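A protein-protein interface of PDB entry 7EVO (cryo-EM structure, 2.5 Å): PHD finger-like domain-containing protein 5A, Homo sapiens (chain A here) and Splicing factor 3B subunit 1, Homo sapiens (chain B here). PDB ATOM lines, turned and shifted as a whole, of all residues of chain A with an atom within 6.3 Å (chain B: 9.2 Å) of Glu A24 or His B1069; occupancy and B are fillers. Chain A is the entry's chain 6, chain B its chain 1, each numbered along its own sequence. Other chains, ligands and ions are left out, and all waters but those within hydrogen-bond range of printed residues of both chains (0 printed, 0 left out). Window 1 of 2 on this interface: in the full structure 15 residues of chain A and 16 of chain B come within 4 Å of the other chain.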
ATOM      1  N   LEU A  22      20.998   4.095  -7.492  1.00  0.00           N
ATOM      2  CA  LEU A  22      22.381   3.804  -7.142  1.00  0.00           C
ATOM      3  C   LEU A  22      22.596   2.299  -7.138  1.00  0.00           C
ATOM      4  O   LEU A  22      21.662   1.532  -6.893  1.00  0.00           O
ATOM      5  CB  LEU A  22      22.753   4.388  -5.772  1.00  0.00           C
ATOM      6  CG  LEU A  22      22.977   5.899  -5.728  1.00  0.00           C
ATOM      7  CD1 LEU A  22      23.225   6.379  -4.310  1.00  0.00           C
ATOM      8  CD2 LEU A  22      24.123   6.288  -6.634  1.00  0.00           C
ATOM      9  N   CYS A  23      23.829   1.882  -7.407  1.00  0.00           N
ATOM     10  CA  CYS A  23      24.150   0.464  -7.439  1.00  0.00           C
ATOM     11  C   CYS A  23      24.627  -0.012  -6.069  1.00  0.00           C
ATOM     12  O   CYS A  23      24.667   0.743  -5.094  1.00  0.00           O
ATOM     13  CB  CYS A  23      25.211   0.173  -8.499  1.00  0.00           C
ATOM     14  SG  CYS A  23      26.887   0.648  -8.044  1.00  0.00           S
ATOM     15  N   GLU A  24      24.987  -1.296  -6.006  1.00  0.00           N
ATOM     16  CA  GLU A  24      25.442  -1.890  -4.753  1.00  0.00           C
ATOM     17  C   GLU A  24      26.758  -1.297  -4.273  1.00  0.00           C
ATOM     18  O   GLU A  24      27.030  -1.307  -3.068  1.00  0.00           O
ATOM     19  CB  GLU A  24      25.584  -3.404  -4.921  1.00  0.00           C
ATOM     20  CG  GLU A  24      24.470  -4.208  -4.281  1.00  0.00           C
ATOM     21  CD  GLU A  24      24.628  -4.330  -2.780  1.00  0.00           C
ATOM     22  OE1 GLU A  24      25.758  -4.598  -2.319  1.00  0.00           O
ATOM     23  OE2 GLU A  24      23.622  -4.159  -2.059  1.00  0.00           O
ATOM     24  N   LYS A  25      27.581  -0.782  -5.186  1.00  0.00           N
ATOM     25  CA  LYS A  25      28.872  -0.230  -4.793  1.00  0.00           C
ATOM     26  C   LYS A  25      28.753   1.233  -4.376  1.00  0.00           C
ATOM     27  O   LYS A  25      29.511   1.703  -3.519  1.00  0.00           O
ATOM     28  CB  LYS A  25      29.870  -0.400  -5.939  1.00  0.00           C
ATOM     29  CG  LYS A  25      31.248   0.177  -5.682  1.00  0.00           C
ATOM     30  CD  LYS A  25      31.979   0.448  -6.988  1.00  0.00           C
ATOM     31  CE  LYS A  25      31.162   1.344  -7.905  1.00  0.00           C
ATOM     32  NZ  LYS A  25      31.890   1.674  -9.160  1.00  0.00           N
ATOM     33  N   CYS A  26      27.805   1.966  -4.958  1.00  0.00           N
ATOM     34  CA  CYS A  26      27.640   3.394  -4.716  1.00  0.00           C
ATOM     35  C   CYS A  26      26.466   3.714  -3.799  1.00  0.00           C
ATOM     36  O   CYS A  26      26.039   4.871  -3.749  1.00  0.00           O
ATOM     37  CB  CYS A  26      27.463   4.134  -6.043  1.00  0.00           C
ATOM     38  SG  CYS A  26      28.762   3.850  -7.258  1.00  0.00           S
ATOM     39  N   ASP A  27      25.948   2.724  -3.070  1.00  0.00           N
ATOM     40  CA  ASP A  27      24.617   2.828  -2.471  1.00  0.00           C
ATOM     41  C   ASP A  27      24.490   4.031  -1.537  1.00  0.00           C
ATOM     42  O   ASP A  27      23.463   4.717  -1.532  1.00  0.00           O
ATOM     43  CB  ASP A  27      24.287   1.533  -1.730  1.00  0.00           C
ATOM     44  CG  ASP A  27      22.809   1.391  -1.433  1.00  0.00           C
ATOM     45  OD1 ASP A  27      22.047   2.337  -1.709  1.00  0.00           O
ATOM     46  OD2 ASP A  27      22.405   0.327  -0.921  1.00  0.00           O
ATOM     47  N   GLY A  28      25.518   4.307  -0.736  1.00  0.00           N
ATOM     48  CA  GLY A  28      25.378   5.349   0.272  1.00  0.00           C
ATOM     49  C   GLY A  28      25.898   6.704  -0.174  1.00  0.00           C
ATOM     50  O   GLY A  28      25.836   7.678   0.581  1.00  0.00           O
ATOM     51  N   PRO A  64      23.760  -1.716 -12.678  1.00  0.00           N
ATOM     52  CA  PRO A  64      22.349  -1.942 -12.339  1.00  0.00           C
ATOM     53  C   PRO A  64      21.969  -1.318 -11.005  1.00  0.00           C
ATOM     54  O   PRO A  64      22.587  -1.609  -9.977  1.00  0.00           O
ATOM     55  CB  PRO A  64      22.237  -3.471 -12.299  1.00  0.00           C
ATOM     56  CG  PRO A  64      23.617  -3.940 -12.014  1.00  0.00           C
ATOM     57  CD  PRO A  64      24.541  -2.964 -12.675  1.00  0.00           C
ATOM     58  N   GLY A  65      20.949  -0.461 -11.010  1.00  0.00           N
ATOM     59  CA  GLY A  65      20.553   0.231  -9.794  1.00  0.00           C
ATOM     60  C   GLY A  65      19.839  -0.695  -8.821  1.00  0.00           C
ATOM     61  O   GLY A  65      19.145  -1.631  -9.213  1.00  0.00           O
ATOM     62  N   VAL A  66      20.026  -0.422  -7.532  1.00  0.00           N
ATOM     63  CA  VAL A  66      19.373  -1.188  -6.475  1.00  0.00           C
ATOM     64  C   VAL A  66      18.623  -0.313  -5.482  1.00  0.00           C
ATOM     65  O   VAL A  66      17.721  -0.820  -4.800  1.00  0.00           O
ATOM     66  CB  VAL A  66      20.376  -2.090  -5.722  1.00  0.00           C
ATOM     67  CG1 VAL A  66      20.921  -3.170  -6.642  1.00  0.00           C
ATOM     68  CG2 VAL A  66      21.501  -1.264  -5.133  1.00  0.00           C
ATOM     69  N   ARG B1027      32.636 -14.237   5.964  1.00  0.00           N
ATOM     70  CA  ARG B1027      32.564 -13.388   4.785  1.00  0.00           C
ATOM     71  C   ARG B1027      31.198 -13.374   4.112  1.00  0.00           C
ATOM     72  O   ARG B1027      31.071 -12.791   3.029  1.00  0.00           O
ATOM     73  CB  ARG B1027      33.627 -13.808   3.761  1.00  0.00           C
ATOM     74  CG  ARG B1027      34.974 -13.141   3.984  1.00  0.00           C
ATOM     75  CD  ARG B1027      34.866 -11.630   3.846  1.00  0.00           C
ATOM     76  NE  ARG B1027      35.694 -10.933   4.824  1.00  0.00           N
ATOM     77  CZ  ARG B1027      35.402  -9.743   5.338  1.00  0.00           C
ATOM     78  NH1 ARG B1027      36.214  -9.185   6.225  1.00  0.00           N
ATOM     79  NH2 ARG B1027      34.297  -9.110   4.969  1.00  0.00           N
ATOM     80  N   GLU B1029      27.320 -12.039   3.852  1.00  0.00           N
ATOM     81  CA  GLU B1029      26.757 -10.735   4.189  1.00  0.00           C
ATOM     82  C   GLU B1029      25.684 -10.851   5.265  1.00  0.00           C
ATOM     83  O   GLU B1029      25.649 -10.053   6.210  1.00  0.00           O
ATOM     84  CB  GLU B1029      26.192 -10.074   2.932  1.00  0.00           C
ATOM     85  CG  GLU B1029      27.106 -10.184   1.725  1.00  0.00           C
ATOM     86  CD  GLU B1029      28.205  -9.143   1.736  1.00  0.00           C
ATOM     87  OE1 GLU B1029      27.968  -8.034   2.257  1.00  0.00           O
ATOM     88  OE2 GLU B1029      29.307  -9.432   1.224  1.00  0.00           O
ATOM     89  N   GLN B1032      27.324 -11.752   8.591  1.00  0.00           N
ATOM     90  CA  GLN B1032      28.026 -10.595   9.136  1.00  0.00           C
ATOM     91  C   GLN B1032      27.050  -9.593   9.732  1.00  0.00           C
ATOM     92  O   GLN B1032      27.238  -9.119  10.859  1.00  0.00           O
ATOM     93  CB  GLN B1032      28.870  -9.936   8.049  1.00  0.00           C
ATOM     94  CG  GLN B1032      30.321 -10.360   8.058  1.00  0.00           C
ATOM     95  CD  GLN B1032      31.154  -9.619   7.036  1.00  0.00           C
ATOM     96  OE1 GLN B1032      30.691  -9.324   5.934  1.00  0.00           O
ATOM     97  NE2 GLN B1032      32.396  -9.319   7.391  1.00  0.00           N
ATOM     98  N   GLU B1033      26.000  -9.251   8.984  1.00  0.00           N
ATOM     99  CA  GLU B1033      25.045  -8.257   9.460  1.00  0.00           C
ATOM    100  C   GLU B1033      24.365  -8.717  10.743  1.00  0.00           C
ATOM    101  O   GLU B1033      24.253  -7.950  11.708  1.00  0.00           O
ATOM    102  CB  GLU B1033      24.012  -7.964   8.374  1.00  0.00           C
ATOM    103  CG  GLU B1033      23.017  -6.882   8.746  1.00  0.00           C
ATOM    104  CD  GLU B1033      22.094  -6.532   7.600  1.00  0.00           C
ATOM    105  OE1 GLU B1033      22.397  -6.922   6.453  1.00  0.00           O
ATOM    106  OE2 GLU B1033      21.065  -5.868   7.844  1.00  0.00           O
ATOM    107  N   GLU B1064      37.787  -2.540  10.816  1.00  0.00           N
ATOM    108  CA  GLU B1064      37.984  -2.919   9.422  1.00  0.00           C
ATOM    109  C   GLU B1064      36.675  -3.091   8.664  1.00  0.00           C
ATOM    110  O   GLU B1064      36.694  -3.151   7.431  1.00  0.00           O
ATOM    111  CB  GLU B1064      38.799  -4.208   9.339  1.00  0.00           C
ATOM    112  CG  GLU B1064      40.294  -4.001   9.498  1.00  0.00           C
ATOM    113  CD  GLU B1064      40.696  -3.720  10.933  1.00  0.00           C
ATOM    114  OE1 GLU B1064      41.687  -2.990  11.137  1.00  0.00           O
ATOM    115  OE2 GLU B1064      40.025  -4.232  11.854  1.00  0.00           O
ATOM    116  N   LEU B1065      35.543  -3.172   9.361  1.00  0.00           N
ATOM    117  CA  LEU B1065      34.272  -3.359   8.670  1.00  0.00           C
ATOM    118  C   LEU B1065      33.667  -2.053   8.177  1.00  0.00           C
ATOM    119  O   LEU B1065      32.656  -2.094   7.467  1.00  0.00           O
ATOM    120  CB  LEU B1065      33.285  -4.088   9.580  1.00  0.00           C
ATOM    121  CG  LEU B1065      33.506  -5.600   9.659  1.00  0.00           C
ATOM    122  CD1 LEU B1065      32.586  -6.229  10.682  1.00  0.00           C
ATOM    123  CD2 LEU B1065      33.309  -6.239   8.297  1.00  0.00           C
ATOM    124  N   LEU B1066      34.249  -0.905   8.525  1.00  0.00           N
ATOM    125  CA  LEU B1066      33.774   0.362   7.984  1.00  0.00           C
ATOM    126  C   LEU B1066      34.121   0.530   6.509  1.00  0.00           C
ATOM    127  O   LEU B1066      33.709   1.521   5.899  1.00  0.00           O
ATOM    128  CB  LEU B1066      34.349   1.526   8.793  1.00  0.00           C
ATOM    129  CG  LEU B1066      33.935   1.585  10.264  1.00  0.00           C
ATOM    130  CD1 LEU B1066      34.725   2.646  11.006  1.00  0.00           C
ATOM    131  CD2 LEU B1066      32.446   1.842  10.391  1.00  0.00           C
ATOM    132  N   LYS B1067      34.866  -0.408   5.927  1.00  0.00           N
ATOM    133  CA  LYS B1067      35.215  -0.379   4.513  1.00  0.00           C
ATOM    134  C   LYS B1067      34.338  -1.290   3.669  1.00  0.00           C
ATOM    135  O   LYS B1067      34.580  -1.411   2.464  1.00  0.00           O
ATOM    136  CB  LYS B1067      36.679  -0.784   4.313  1.00  0.00           C
ATOM    137  CG  LYS B1067      37.538  -0.678   5.555  1.00  0.00           C
ATOM    138  CD  LYS B1067      38.992  -0.407   5.205  1.00  0.00           C
ATOM    139  CE  LYS B1067      39.684  -1.662   4.706  1.00  0.00           C
ATOM    140  NZ  LYS B1067      41.123  -1.425   4.429  1.00  0.00           N
ATOM    141  N   ALA B1068      33.347  -1.944   4.272  1.00  0.00           N
ATOM    142  CA  ALA B1068      32.520  -2.919   3.576  1.00  0.00           C
ATOM    143  C   ALA B1068      31.864  -2.316   2.341  1.00  0.00           C
ATOM    144  O   ALA B1068      31.452  -1.154   2.343  1.00  0.00           O
ATOM    145  CB  ALA B1068      31.450  -3.462   4.524  1.00  0.00           C
ATOM    146  N   HIS B1069      31.772  -3.123   1.283  1.00  0.00           N
ATOM    147  CA  HIS B1069      31.118  -2.698   0.054  1.00  0.00           C
ATOM    148  C   HIS B1069      29.606  -2.591   0.195  1.00  0.00           C
ATOM    149  O   HIS B1069      28.953  -2.076  -0.716  1.00  0.00           O
ATOM    150  CB  HIS B1069      31.458  -3.667  -1.081  1.00  0.00           C
ATOM    151  CG  HIS B1069      32.924  -3.923  -1.242  1.00  0.00           C
ATOM    152  ND1 HIS B1069      33.771  -3.035  -1.869  1.00  0.00           N
ATOM    153  CD2 HIS B1069      33.693  -4.970  -0.858  1.00  0.00           C
ATOM    154  CE1 HIS B1069      34.999  -3.523  -1.866  1.00  0.00           C
ATOM    155  NE2 HIS B1069      34.979  -4.696  -1.258  1.00  0.00           N
ATOM    156  N   LYS B1070      29.037  -3.059   1.303  1.00  0.00           N
ATOM    157  CA  LYS B1070      27.594  -3.123   1.490  1.00  0.00           C
ATOM    158  C   LYS B1070      27.164  -2.109   2.541  1.00  0.00           C
ATOM    159  O   LYS B1070      27.888  -1.870   3.513  1.00  0.00           O
ATOM    160  CB  LYS B1070      27.161  -4.534   1.896  1.00  0.00           C
ATOM    161  CG  LYS B1070      26.834  -5.442   0.719  1.00  0.00           C
ATOM    162  CD  LYS B1070      28.073  -5.741  -0.117  1.00  0.00           C
ATOM    163  CE  LYS B1070      27.914  -7.008  -0.936  1.00  0.00           C
ATOM    164  NZ  LYS B1070      29.194  -7.768  -1.016  1.00  0.00           N
ATOM    165  N   LYS B1071      25.982  -1.522   2.344  1.00  0.00           N
ATOM    166  CA  LYS B1071      25.549  -0.412   3.188  1.00  0.00           C
ATOM    167  C   LYS B1071      25.016  -0.886   4.534  1.00  0.00           C
ATOM    168  O   LYS B1071      25.187  -0.195   5.547  1.00  0.00           O
ATOM    169  CB  LYS B1071      24.491   0.406   2.450  1.00  0.00           C
ATOM    170  CG  LYS B1071      24.277   1.800   3.002  1.00  0.00           C
ATOM    171  CD  LYS B1071      22.801   2.109   3.152  1.00  0.00           C
ATOM    172  CE  LYS B1071      22.204   2.571   1.837  1.00  0.00           C
ATOM    173  NZ  LYS B1071      20.940   3.325   2.041  1.00  0.00           N
ATOM    174  N   ALA B1072      24.378  -2.059   4.574  1.00  0.00           N
ATOM    175  CA  ALA B1072      23.829  -2.552   5.834  1.00  0.00           C
ATOM    176  C   ALA B1072      24.937  -2.946   6.801  1.00  0.00           C
ATOM    177  O   ALA B1072      24.818  -2.728   8.014  1.00  0.00           O
ATOM    178  CB  ALA B1072      22.898  -3.734   5.570  1.00  0.00           C
ATOM    179  N   ILE B1073      26.023  -3.521   6.280  1.00  0.00           N
ATOM    180  CA  ILE B1073      27.177  -3.835   7.114  1.00  0.00           C
ATOM    181  C   ILE B1073      27.731  -2.569   7.752  1.00  0.00           C
ATOM    182  O   ILE B1073      28.013  -2.536   8.955  1.00  0.00           O
ATOM    183  CB  ILE B1073      28.251  -4.570   6.291  1.00  0.00           C
ATOM    184  CG1 ILE B1073      27.667  -5.823   5.643  1.00  0.00           C
ATOM    185  CG2 ILE B1073      29.427  -4.951   7.171  1.00  0.00           C
ATOM    186  CD1 ILE B1073      27.074  -6.791   6.630  1.00  0.00           C
ATOM    187  N   ARG B1074      27.887  -1.504   6.960  1.00  0.00           N
ATOM    188  CA  ARG B1074      28.420  -0.255   7.493  1.00  0.00           C
ATOM    189  C   ARG B1074      27.479   0.359   8.523  1.00  0.00           C
ATOM    190  O   ARG B1074      27.927   0.870   9.555  1.00  0.00           O
ATOM    191  CB  ARG B1074      28.686   0.729   6.356  1.00  0.00           C
ATOM    192  CG  ARG B1074      29.750   0.271   5.380  1.00  0.00           C
ATOM    193  CD  ARG B1074      30.193   1.408   4.477  1.00  0.00           C
ATOM    194  NE  ARG B1074      29.069   2.005   3.761  1.00  0.00           N
ATOM    195  CZ  ARG B1074      28.794   1.780   2.481  1.00  0.00           C
ATOM    196  NH1 ARG B1074      29.565   0.970   1.769  1.00  0.00           N
ATOM    197  NH2 ARG B1074      27.750   2.364   1.912  1.00  0.00           N
ATOM    198  N   GLN B1107      43.630   3.711   3.859  1.00  0.00           N
ATOM    199  CA  GLN B1107      42.243   3.328   4.108  1.00  0.00           C
ATOM    200  C   GLN B1107      41.985   3.107   5.593  1.00  0.00           C
ATOM    201  O   GLN B1107      40.930   3.490   6.117  1.00  0.00           O
ATOM    202  CB  GLN B1107      41.900   2.076   3.305  1.00  0.00           C
ATOM    203  CG  GLN B1107      41.068   2.358   2.067  1.00  0.00           C
ATOM    204  CD  GLN B1107      39.611   2.632   2.386  1.00  0.00           C
ATOM    205  OE1 GLN B1107      39.187   3.786   2.469  1.00  0.00           O
ATOM    206  NE2 GLN B1107      38.833   1.571   2.556  1.00  0.00           N
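Among the printed residues, merely in contact across the chains: Glu A24 with Lys B1070 (3.3 Å), Asp A27 with Lys B1071 (3.5 Å) and Gly A28 with Arg B1074 (3.97 Å).
The backbone carbonyl oxygen of Glu A24 lies close to the backbone carbonyl oxygen of His B1069 (3.1 Å).
The side-chain carboxylate (OE2) of Glu B1029 is in salt-bridge range of the side-chain amino group (NZ) of Lys B1070 (2.8 Å).
The backbone carbonyl oxygen (O) of Ala B1068 lies within hydrogen-bond range of the guanidinium group (NH1) of Arg B1074 (2.9 Å).
Of the 16 printed residues of chain B, 4 touch a printed residue of chain A.
Along chain B the printed residues that touch a printed residue of chain A span positions 1069 to 1074.
Printed residues of chain A that touch a printed residue of chain B: Glu A24, Asp A27 and Gly A28.
Along chain A the printed residues that touch a printed residue of chain B span positions 24 to 28.
Among the printed residues, no Asp or Glu carboxylate lies within 4 Å of a Lys or Arg side-chain nitrogen of the other chain.
Glu A24 touches just these residues of chain B: His B1069 and Lys B1070.
His B1069 touches one residue of chain A.
Of the printed residues of chain A, Arg B1074 touches Gly A28.
Of the printed residues of chain B, Asp A27 touches Lys B1071.
Printed residues of chain A within 4 Å of Lys B1071: Asp A27.
Of the printed residues of chain A, Lys B1070 touches Glu A24 (3.3 Å).
Ala B1072 touches none of the printed residues of chain A.
Val A66 touches none of the printed residues of chain B.
The nearest residue of chain B that does not touch Glu A24 is Lys B1071 (5.5 Å).
The nearest residue of chain A that does not touch His B1069 is Lys A25 (4.5 Å).
The nearest printed residue of chain B that does not touch Gly A28 is Lys B1071 (4.5 Å).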
